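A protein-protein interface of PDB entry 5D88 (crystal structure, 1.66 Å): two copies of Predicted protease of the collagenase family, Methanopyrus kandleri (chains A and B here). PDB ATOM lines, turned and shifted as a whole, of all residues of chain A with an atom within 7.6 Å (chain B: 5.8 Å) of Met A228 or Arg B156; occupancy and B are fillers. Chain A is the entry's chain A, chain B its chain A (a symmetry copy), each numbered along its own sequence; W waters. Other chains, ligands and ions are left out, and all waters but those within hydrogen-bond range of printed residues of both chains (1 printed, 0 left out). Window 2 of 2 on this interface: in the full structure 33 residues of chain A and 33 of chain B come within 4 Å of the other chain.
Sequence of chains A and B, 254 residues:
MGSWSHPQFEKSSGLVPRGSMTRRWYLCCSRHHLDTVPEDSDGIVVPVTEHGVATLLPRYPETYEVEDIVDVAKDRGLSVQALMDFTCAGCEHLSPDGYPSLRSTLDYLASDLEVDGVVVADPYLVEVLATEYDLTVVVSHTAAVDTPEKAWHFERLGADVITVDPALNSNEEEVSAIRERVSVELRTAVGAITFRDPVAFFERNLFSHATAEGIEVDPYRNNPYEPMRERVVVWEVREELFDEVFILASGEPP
Among the printed residues, pairs that only touch across the chains: Phe A202 with Pro B123, Pro A198 with His B153, Pro A224 with Tyr B124, Met A228 with Tyr B124, Val A199 with Pro B123, Met A228 with Pro B123 and Met A228 with Glu B127.
Of the 12 printed residues of chain A, 5 touch a printed residue of chain B. Along chain A the printed residues that touch a printed residue of chain B span positions 198 to 228. Of the 12 printed residues of chain B, 5 touch a printed residue of chain A. Along chain B the printed residues that touch a printed residue of chain A span positions 123 to 156. Among the printed residues, 8 pairs touch across the chains.
Water W1 lies within hydrogen-bond range of O of Pro A224 (2.6 Å) and OE1 of Glu B127 (3.1 Å).
O of Met A228 sits at hydrogen-bond distance from NH2 of Arg B156, 2.8 Å away.
The guanidinium group (NH2) of Arg B156 is in hydrogen-bond range of a ring nitrogen (ND1) of His B153.
Printed residues of chain B within 4 Å of Pro A224: Tyr B124. Met A228 touches just these residues of chain B: Pro B123, Tyr B124, Glu B127 and Arg B156. Printed residues of chain A within 4 Å of Glu B127: Met A228 (3.9 Å). Arg B156 touches just one residue of chain A: Met A228. Gly B158 touches none of the printed residues of chain A. The nearest residue of chain B that does not touch Met A228 is Leu B157 (4.2 Å).
No position is printed for both chains.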
ATOM      1  N   PRO A 198      -2.098   2.128  -8.054  1.00  0.00           N
ATOM      2  CA  PRO A 198      -2.727   0.794  -8.023  1.00  0.00           C
ATOM      3  C   PRO A 198      -2.423  -0.057  -6.780  1.00  0.00           C
ATOM      4  O   PRO A 198      -3.256  -0.880  -6.394  1.00  0.00           O
ATOM      5  CB  PRO A 198      -2.180   0.134  -9.292  1.00  0.00           C
ATOM      6  CG  PRO A 198      -0.867   0.882  -9.582  1.00  0.00           C
ATOM      7  CD  PRO A 198      -1.219   2.308  -9.231  1.00  0.00           C
ATOM      8  N   VAL A 199      -1.264   0.085  -6.144  1.00  0.00           N
ATOM      9  CA  VAL A 199      -0.888  -0.822  -5.064  1.00  0.00           C
ATOM     10  C   VAL A 199      -0.576  -0.091  -3.761  1.00  0.00           C
ATOM     11  O   VAL A 199      -0.235  -0.741  -2.771  1.00  0.00           O
ATOM     12  CB  VAL A 199       0.278  -1.744  -5.475  1.00  0.00           C
ATOM     13  CG1 VAL A 199       0.003  -2.391  -6.825  1.00  0.00           C
ATOM     14  CG2 VAL A 199       1.540  -1.029  -5.511  1.00  0.00           C
ATOM     15  N   PHE A 202      -1.912  -1.466  -0.373  1.00  0.00           N
ATOM     16  CA  PHE A 202      -1.290  -2.666   0.150  1.00  0.00           C
ATOM     17  C   PHE A 202       0.101  -2.366   0.693  1.00  0.00           C
ATOM     18  O   PHE A 202       0.507  -2.920   1.719  1.00  0.00           O
ATOM     19  CB  PHE A 202      -1.241  -3.720  -0.957  1.00  0.00           C
ATOM     20  CG  PHE A 202      -2.602  -4.033  -1.520  1.00  0.00           C
ATOM     21  CD1 PHE A 202      -3.435  -4.927  -0.864  1.00  0.00           C
ATOM     22  CD2 PHE A 202      -3.066  -3.394  -2.660  1.00  0.00           C
ATOM     23  CE1 PHE A 202      -4.695  -5.203  -1.345  1.00  0.00           C
ATOM     24  CE2 PHE A 202      -4.345  -3.652  -3.154  1.00  0.00           C
ATOM     25  CZ  PHE A 202      -5.161  -4.560  -2.496  1.00  0.00           C
ATOM     26  N   ASN A 223      10.565  -5.932  -0.179  1.00  0.00           N
ATOM     27  CA  ASN A 223       9.303  -5.235  -0.425  1.00  0.00           C
ATOM     28  C   ASN A 223       8.741  -5.709  -1.757  1.00  0.00           C
ATOM     29  O   ASN A 223       9.275  -5.334  -2.804  1.00  0.00           O
ATOM     30  CB  ASN A 223       9.497  -3.724  -0.445  1.00  0.00           C
ATOM     31  CG  ASN A 223       8.188  -2.973  -0.755  1.00  0.00           C
ATOM     32  OD1 ASN A 223       7.148  -3.581  -0.981  1.00  0.00           O
ATOM     33  ND2 ASN A 223       8.244  -1.655  -0.735  1.00  0.00           N
ATOM     34  N   PRO A 224       7.691  -6.527  -1.776  1.00  0.00           N
ATOM     35  CA  PRO A 224       7.221  -7.078  -3.055  1.00  0.00           C
ATOM     36  C   PRO A 224       6.540  -6.058  -3.943  1.00  0.00           C
ATOM     37  O   PRO A 224       6.367  -6.319  -5.145  1.00  0.00           O
ATOM     38  CB  PRO A 224       6.252  -8.180  -2.621  1.00  0.00           C
ATOM     39  CG  PRO A 224       5.761  -7.737  -1.276  1.00  0.00           C
ATOM     40  CD  PRO A 224       6.897  -7.002  -0.633  1.00  0.00           C
ATOM     41  N   TYR A 225       6.133  -4.929  -3.386  1.00  0.00           N
ATOM     42  CA  TYR A 225       5.437  -3.884  -4.120  1.00  0.00           C
ATOM     43  C   TYR A 225       6.405  -2.931  -4.799  1.00  0.00           C
ATOM     44  O   TYR A 225       6.022  -2.260  -5.760  1.00  0.00           O
ATOM     45  CB  TYR A 225       4.496  -3.125  -3.153  1.00  0.00           C
ATOM     46  CG  TYR A 225       3.571  -4.061  -2.411  1.00  0.00           C
ATOM     47  CD1 TYR A 225       2.635  -4.832  -3.087  1.00  0.00           C
ATOM     48  CD2 TYR A 225       3.660  -4.217  -1.041  1.00  0.00           C
ATOM     49  CE1 TYR A 225       1.822  -5.741  -2.413  1.00  0.00           C
ATOM     50  CE2 TYR A 225       2.837  -5.125  -0.374  1.00  0.00           C
ATOM     51  CZ  TYR A 225       1.935  -5.880  -1.073  1.00  0.00           C
ATOM     52  OH  TYR A 225       1.125  -6.774  -0.408  1.00  0.00           O
ATOM     53  N   GLU A 226       7.668  -2.901  -4.361  1.00  0.00           N
ATOM     54  CA  GLU A 226       8.631  -1.946  -4.916  1.00  0.00           C
ATOM     55  C   GLU A 226       8.833  -2.118  -6.421  1.00  0.00           C
ATOM     56  O   GLU A 226       8.786  -1.109  -7.150  1.00  0.00           O
ATOM     57  CB  GLU A 226       9.934  -2.076  -4.112  1.00  0.00           C
ATOM     58  CG  GLU A 226      11.201  -1.395  -4.647  1.00  0.00           C
ATOM     59  CD  GLU A 226      11.211   0.130  -4.592  1.00  0.00           C
ATOM     60  OE1 GLU A 226      10.656   0.758  -3.659  1.00  0.00           O
ATOM     61  OE2 GLU A 226      11.846   0.701  -5.511  1.00  0.00           O
ATOM     62  N   PRO A 227       9.043  -3.322  -6.957  1.00  0.00           N
ATOM     63  CA  PRO A 227       9.245  -3.461  -8.411  1.00  0.00           C
ATOM     64  C   PRO A 227       7.981  -3.358  -9.258  1.00  0.00           C
ATOM     65  O   PRO A 227       8.078  -3.416 -10.494  1.00  0.00           O
ATOM     66  CB  PRO A 227       9.853  -4.858  -8.545  1.00  0.00           C
ATOM     67  CG  PRO A 227       9.515  -5.569  -7.305  1.00  0.00           C
ATOM     68  CD  PRO A 227       9.260  -4.582  -6.234  1.00  0.00           C
ATOM     69  N   MET A 228       6.809  -3.216  -8.648  1.00  0.00           N
ATOM     70  CA  MET A 228       5.560  -3.357  -9.395  1.00  0.00           C
ATOM     71  C   MET A 228       5.210  -2.159 -10.266  1.00  0.00           C
ATOM     72  O   MET A 228       4.580  -2.348 -11.315  1.00  0.00           O
ATOM     73  CB  MET A 228       4.404  -3.617  -8.432  1.00  0.00           C
ATOM     74  CG  MET A 228       4.388  -5.010  -7.891  1.00  0.00           C
ATOM     75  SD  MET A 228       2.860  -5.290  -6.955  1.00  0.00           S
ATOM     76  CE  MET A 228       3.169  -6.937  -6.351  1.00  0.00           C
ATOM     77  N   ARG A 229       5.551  -0.931  -9.871  1.00  0.00           N
ATOM     78  CA  ARG A 229       5.112   0.211 -10.667  1.00  0.00           C
ATOM     79  C   ARG A 229       5.908   1.452 -10.296  1.00  0.00           C
ATOM     80  O   ARG A 229       6.672   1.466  -9.329  1.00  0.00           O
ATOM     81  CB  ARG A 229       3.606   0.484 -10.483  1.00  0.00           C
ATOM     82  CG  ARG A 229       3.233   1.341  -9.268  1.00  0.00           C
ATOM     83  CD  ARG A 229       3.604   0.703  -7.987  1.00  0.00           C
ATOM     84  NE  ARG A 229       3.002   1.381  -6.824  1.00  0.00           N
ATOM     85  CZ  ARG A 229       3.426   1.241  -5.567  1.00  0.00           C
ATOM     86  NH1 ARG A 229       4.489   0.491  -5.284  1.00  0.00           N
ATOM     87  NH2 ARG A 229       2.809   1.870  -4.594  1.00  0.00           N
ATOM     88  N   GLU A 230       5.686   2.504 -11.087  1.00  0.00           N
ATOM     89  CA  GLU A 230       6.118   3.860 -10.771  1.00  0.00           C
ATOM     90  C   GLU A 230       5.049   4.493  -9.894  1.00  0.00           C
ATOM     91  O   GLU A 230       3.900   4.654 -10.324  1.00  0.00           O
ATOM     92  CB  GLU A 230       6.322   4.682 -12.051  1.00  0.00           C
ATOM     93  CG  GLU A 230       6.871   6.103 -11.850  1.00  0.00           C
ATOM     94  CD  GLU A 230       8.326   6.138 -11.344  1.00  0.00           C
ATOM     95  OE1 GLU A 230       9.044   5.120 -11.478  1.00  0.00           O
ATOM     96  OE2 GLU A 230       8.752   7.192 -10.811  1.00  0.00           O
ATOM     97  N   ARG A 231       5.408   4.806  -8.655  1.00  0.00           N
ATOM     98  CA  ARG A 231       4.424   5.315  -7.716  1.00  0.00           C
ATOM     99  C   ARG A 231       3.798   6.617  -8.212  1.00  0.00           C
ATOM    100  O   ARG A 231       4.468   7.477  -8.783  1.00  0.00           O
ATOM    101  CB  ARG A 231       5.075   5.512  -6.346  1.00  0.00           C
ATOM    102  CG  ARG A 231       5.443   4.187  -5.675  1.00  0.00           C
ATOM    103  CD  ARG A 231       5.752   4.340  -4.192  1.00  0.00           C
ATOM    104  NE  ARG A 231       6.258   3.086  -3.638  1.00  0.00           N
ATOM    105  CZ  ARG A 231       7.501   2.677  -3.819  1.00  0.00           C
ATOM    106  NH1 ARG A 231       8.343   3.450  -4.488  1.00  0.00           N
ATOM    107  NH2 ARG A 231       7.906   1.518  -3.345  1.00  0.00           N
ATOM    108  N   PRO B 123      -2.007  -7.677  -4.559  1.00  0.00           N
ATOM    109  CA  PRO B 123      -1.303  -7.742  -5.847  1.00  0.00           C
ATOM    110  C   PRO B 123      -0.180  -8.763  -5.893  1.00  0.00           C
ATOM    111  O   PRO B 123       0.125  -9.343  -6.952  1.00  0.00           O
ATOM    112  CB  PRO B 123      -0.741  -6.323  -5.995  1.00  0.00           C
ATOM    113  CG  PRO B 123      -1.472  -5.477  -5.100  1.00  0.00           C
ATOM    114  CD  PRO B 123      -2.043  -6.311  -4.008  1.00  0.00           C
ATOM    115  N   TYR B 124       0.484  -8.980  -4.771  1.00  0.00           N
ATOM    116  CA  TYR B 124       1.566  -9.954  -4.774  1.00  0.00           C
ATOM    117  C   TYR B 124       1.025 -11.363  -4.984  1.00  0.00           C
ATOM    118  O   TYR B 124       1.639 -12.172  -5.692  1.00  0.00           O
ATOM    119  CB  TYR B 124       2.339  -9.825  -3.465  1.00  0.00           C
ATOM    120  CG  TYR B 124       3.509 -10.741  -3.284  1.00  0.00           C
ATOM    121  CD1 TYR B 124       4.472 -10.903  -4.275  1.00  0.00           C
ATOM    122  CD2 TYR B 124       3.688 -11.417  -2.088  1.00  0.00           C
ATOM    123  CE1 TYR B 124       5.573 -11.723  -4.064  1.00  0.00           C
ATOM    124  CE2 TYR B 124       4.774 -12.247  -1.884  1.00  0.00           C
ATOM    125  CZ  TYR B 124       5.708 -12.388  -2.871  1.00  0.00           C
ATOM    126  OH  TYR B 124       6.782 -13.207  -2.652  1.00  0.00           O
ATOM    127  N   GLU B 127       0.208 -11.961  -8.617  1.00  0.00           N
ATOM    128  CA  GLU B 127       1.398 -12.234  -9.412  1.00  0.00           C
ATOM    129  C   GLU B 127       1.882 -13.670  -9.214  1.00  0.00           C
ATOM    130  O   GLU B 127       2.213 -14.370 -10.184  1.00  0.00           O
ATOM    131  CB  GLU B 127       2.478 -11.215  -9.039  1.00  0.00           C
ATOM    132  CG  GLU B 127       3.623 -11.103  -9.994  1.00  0.00           C
ATOM    133  CD  GLU B 127       4.511  -9.925  -9.628  1.00  0.00           C
ATOM    134  OE1 GLU B 127       4.808  -9.743  -8.421  1.00  0.00           O
ATOM    135  OE2 GLU B 127       4.881  -9.166 -10.537  1.00  0.00           O
ATOM    136  N   ALA B 151      -7.346  -1.252 -13.016  1.00  0.00           N
ATOM    137  CA  ALA B 151      -7.625  -2.501 -13.711  1.00  0.00           C
ATOM    138  C   ALA B 151      -6.434  -2.928 -14.550  1.00  0.00           C
ATOM    139  O   ALA B 151      -6.067  -4.107 -14.569  1.00  0.00           O
ATOM    140  CB  ALA B 151      -8.861  -2.338 -14.589  1.00  0.00           C
ATOM    141  N   TRP B 152      -5.820  -1.981 -15.251  1.00  0.00           N
ATOM    142  CA  TRP B 152      -4.718  -2.323 -16.147  1.00  0.00           C
ATOM    143  C   TRP B 152      -3.530  -2.895 -15.374  1.00  0.00           C
ATOM    144  O   TRP B 152      -2.888  -3.854 -15.820  1.00  0.00           O
ATOM    145  CB  TRP B 152      -4.313  -1.087 -16.956  1.00  0.00           C
ATOM    146  CG  TRP B 152      -3.262  -1.379 -17.983  1.00  0.00           C
ATOM    147  CD1 TRP B 152      -3.458  -1.832 -19.262  1.00  0.00           C
ATOM    148  CD2 TRP B 152      -1.848  -1.266 -17.816  1.00  0.00           C
ATOM    149  NE1 TRP B 152      -2.256  -1.991 -19.893  1.00  0.00           N
ATOM    150  CE2 TRP B 152      -1.253  -1.656 -19.024  1.00  0.00           C
ATOM    151  CE3 TRP B 152      -1.029  -0.866 -16.763  1.00  0.00           C
ATOM    152  CZ2 TRP B 152       0.125  -1.655 -19.210  1.00  0.00           C
ATOM    153  CZ3 TRP B 152       0.341  -0.872 -16.952  1.00  0.00           C
ATOM    154  CH2 TRP B 152       0.901  -1.259 -18.165  1.00  0.00           C
ATOM    155  N   HIS B 153      -3.226  -2.335 -14.203  1.00  0.00           N
ATOM    156  CA  HIS B 153      -2.128  -2.876 -13.423  1.00  0.00           C
ATOM    157  C   HIS B 153      -2.439  -4.271 -12.904  1.00  0.00           C
ATOM    158  O   HIS B 153      -1.550  -5.137 -12.902  1.00  0.00           O
ATOM    159  CB  HIS B 153      -1.778  -1.907 -12.300  1.00  0.00           C
ATOM    160  CG  HIS B 153      -1.026  -0.702 -12.795  1.00  0.00           C
ATOM    161  ND1 HIS B 153       0.338  -0.716 -13.018  1.00  0.00           N
ATOM    162  CD2 HIS B 153      -1.448   0.537 -13.155  1.00  0.00           C
ATOM    163  CE1 HIS B 153       0.725   0.465 -13.465  1.00  0.00           C
ATOM    164  NE2 HIS B 153      -0.339   1.242 -13.563  1.00  0.00           N
ATOM    165  N   PHE B 154      -3.687  -4.527 -12.473  1.00  0.00           N
ATOM    166  CA  PHE B 154      -3.999  -5.879 -12.020  1.00  0.00           C
ATOM    167  C   PHE B 154      -3.957  -6.876 -13.177  1.00  0.00           C
ATOM    168  O   PHE B 154      -3.514  -8.021 -13.001  1.00  0.00           O
ATOM    169  CB  PHE B 154      -5.352  -5.912 -11.308  1.00  0.00           C
ATOM    170  CG  PHE B 154      -5.271  -5.639  -9.839  1.00  0.00           C
ATOM    171  CD1 PHE B 154      -4.864  -6.621  -8.948  1.00  0.00           C
ATOM    172  CD2 PHE B 154      -5.584  -4.397  -9.343  1.00  0.00           C
ATOM    173  CE1 PHE B 154      -4.806  -6.367  -7.593  1.00  0.00           C
ATOM    174  CE2 PHE B 154      -5.514  -4.140  -7.995  1.00  0.00           C
ATOM    175  CZ  PHE B 154      -5.123  -5.118  -7.123  1.00  0.00           C
ATOM    176  N   GLU B 155      -4.370  -6.458 -14.368  1.00  0.00           N
ATOM    177  CA  GLU B 155      -4.242  -7.319 -15.540  1.00  0.00           C
ATOM    178  C   GLU B 155      -2.779  -7.648 -15.810  1.00  0.00           C
ATOM    179  O   GLU B 155      -2.419  -8.809 -16.057  1.00  0.00           O
ATOM    180  CB  GLU B 155      -4.873  -6.641 -16.759  1.00  0.00           C
ATOM    181  CG  GLU B 155      -4.703  -7.440 -18.051  1.00  0.00           C
ATOM    182  CD  GLU B 155      -5.368  -6.778 -19.255  1.00  0.00           C
ATOM    183  OE1 GLU B 155      -4.962  -5.655 -19.628  1.00  0.00           O
ATOM    184  OE2 GLU B 155      -6.310  -7.380 -19.813  1.00  0.00           O
ATOM    185  N   ARG B 156      -1.919  -6.628 -15.758  1.00  0.00           N
ATOM    186  CA  ARG B 156      -0.499  -6.819 -16.019  1.00  0.00           C
ATOM    187  C   ARG B 156       0.126  -7.778 -15.013  1.00  0.00           C
ATOM    188  O   ARG B 156       1.007  -8.567 -15.374  1.00  0.00           O
ATOM    189  CB  ARG B 156       0.210  -5.467 -16.008  1.00  0.00           C
ATOM    190  CG  ARG B 156       1.666  -5.544 -16.476  1.00  0.00           C
ATOM    191  CD  ARG B 156       2.368  -4.179 -16.506  1.00  0.00           C
ATOM    192  NE  ARG B 156       2.124  -3.396 -15.302  1.00  0.00           N
ATOM    193  CZ  ARG B 156       2.757  -3.576 -14.148  1.00  0.00           C
ATOM    194  NH1 ARG B 156       3.688  -4.518 -14.021  1.00  0.00           N
ATOM    195  NH2 ARG B 156       2.452  -2.811 -13.108  1.00  0.00           N
ATOM    196  N   LEU B 157      -0.350  -7.758 -13.769  1.00  0.00           N
ATOM    197  CA  LEU B 157       0.154  -8.677 -12.760  1.00  0.00           C
ATOM    198  C   LEU B 157      -0.342 -10.096 -12.961  1.00  0.00           C
ATOM    199  O   LEU B 157       0.239 -11.023 -12.378  1.00  0.00           O
ATOM    200  CB  LEU B 157      -0.238  -8.212 -11.361  1.00  0.00           C
ATOM    201  CG  LEU B 157       0.424  -6.940 -10.846  1.00  0.00           C
ATOM    202  CD1 LEU B 157      -0.297  -6.557  -9.560  1.00  0.00           C
ATOM    203  CD2 LEU B 157       1.928  -7.108 -10.596  1.00  0.00           C
ATOM    204  N   GLY B 158      -1.398 -10.286 -13.758  1.00  0.00           N
ATOM    205  CA  GLY B 158      -1.847 -11.621 -14.111  1.00  0.00           C
ATOM    206  C   GLY B 158      -3.303 -11.945 -13.820  1.00  0.00           C
ATOM    207  O   GLY B 158      -3.699 -13.111 -13.886  1.00  0.00           O
ATOM    208  N   ALA B 159      -4.122 -10.952 -13.514  1.00  0.00           N
ATOM    209  CA  ALA B 159      -5.525 -11.246 -13.273  1.00  0.00           C
ATOM    210  C   ALA B 159      -6.183 -11.794 -14.530  1.00  0.00           C
ATOM    211  O   ALA B 159      -5.916 -11.330 -15.641  1.00  0.00           O
ATOM    212  CB  ALA B 159      -6.270  -9.996 -12.800  1.00  0.00           C
HETATM  213  O   HOH W   1       6.930  -8.252  -6.801  1.00  0.00           O
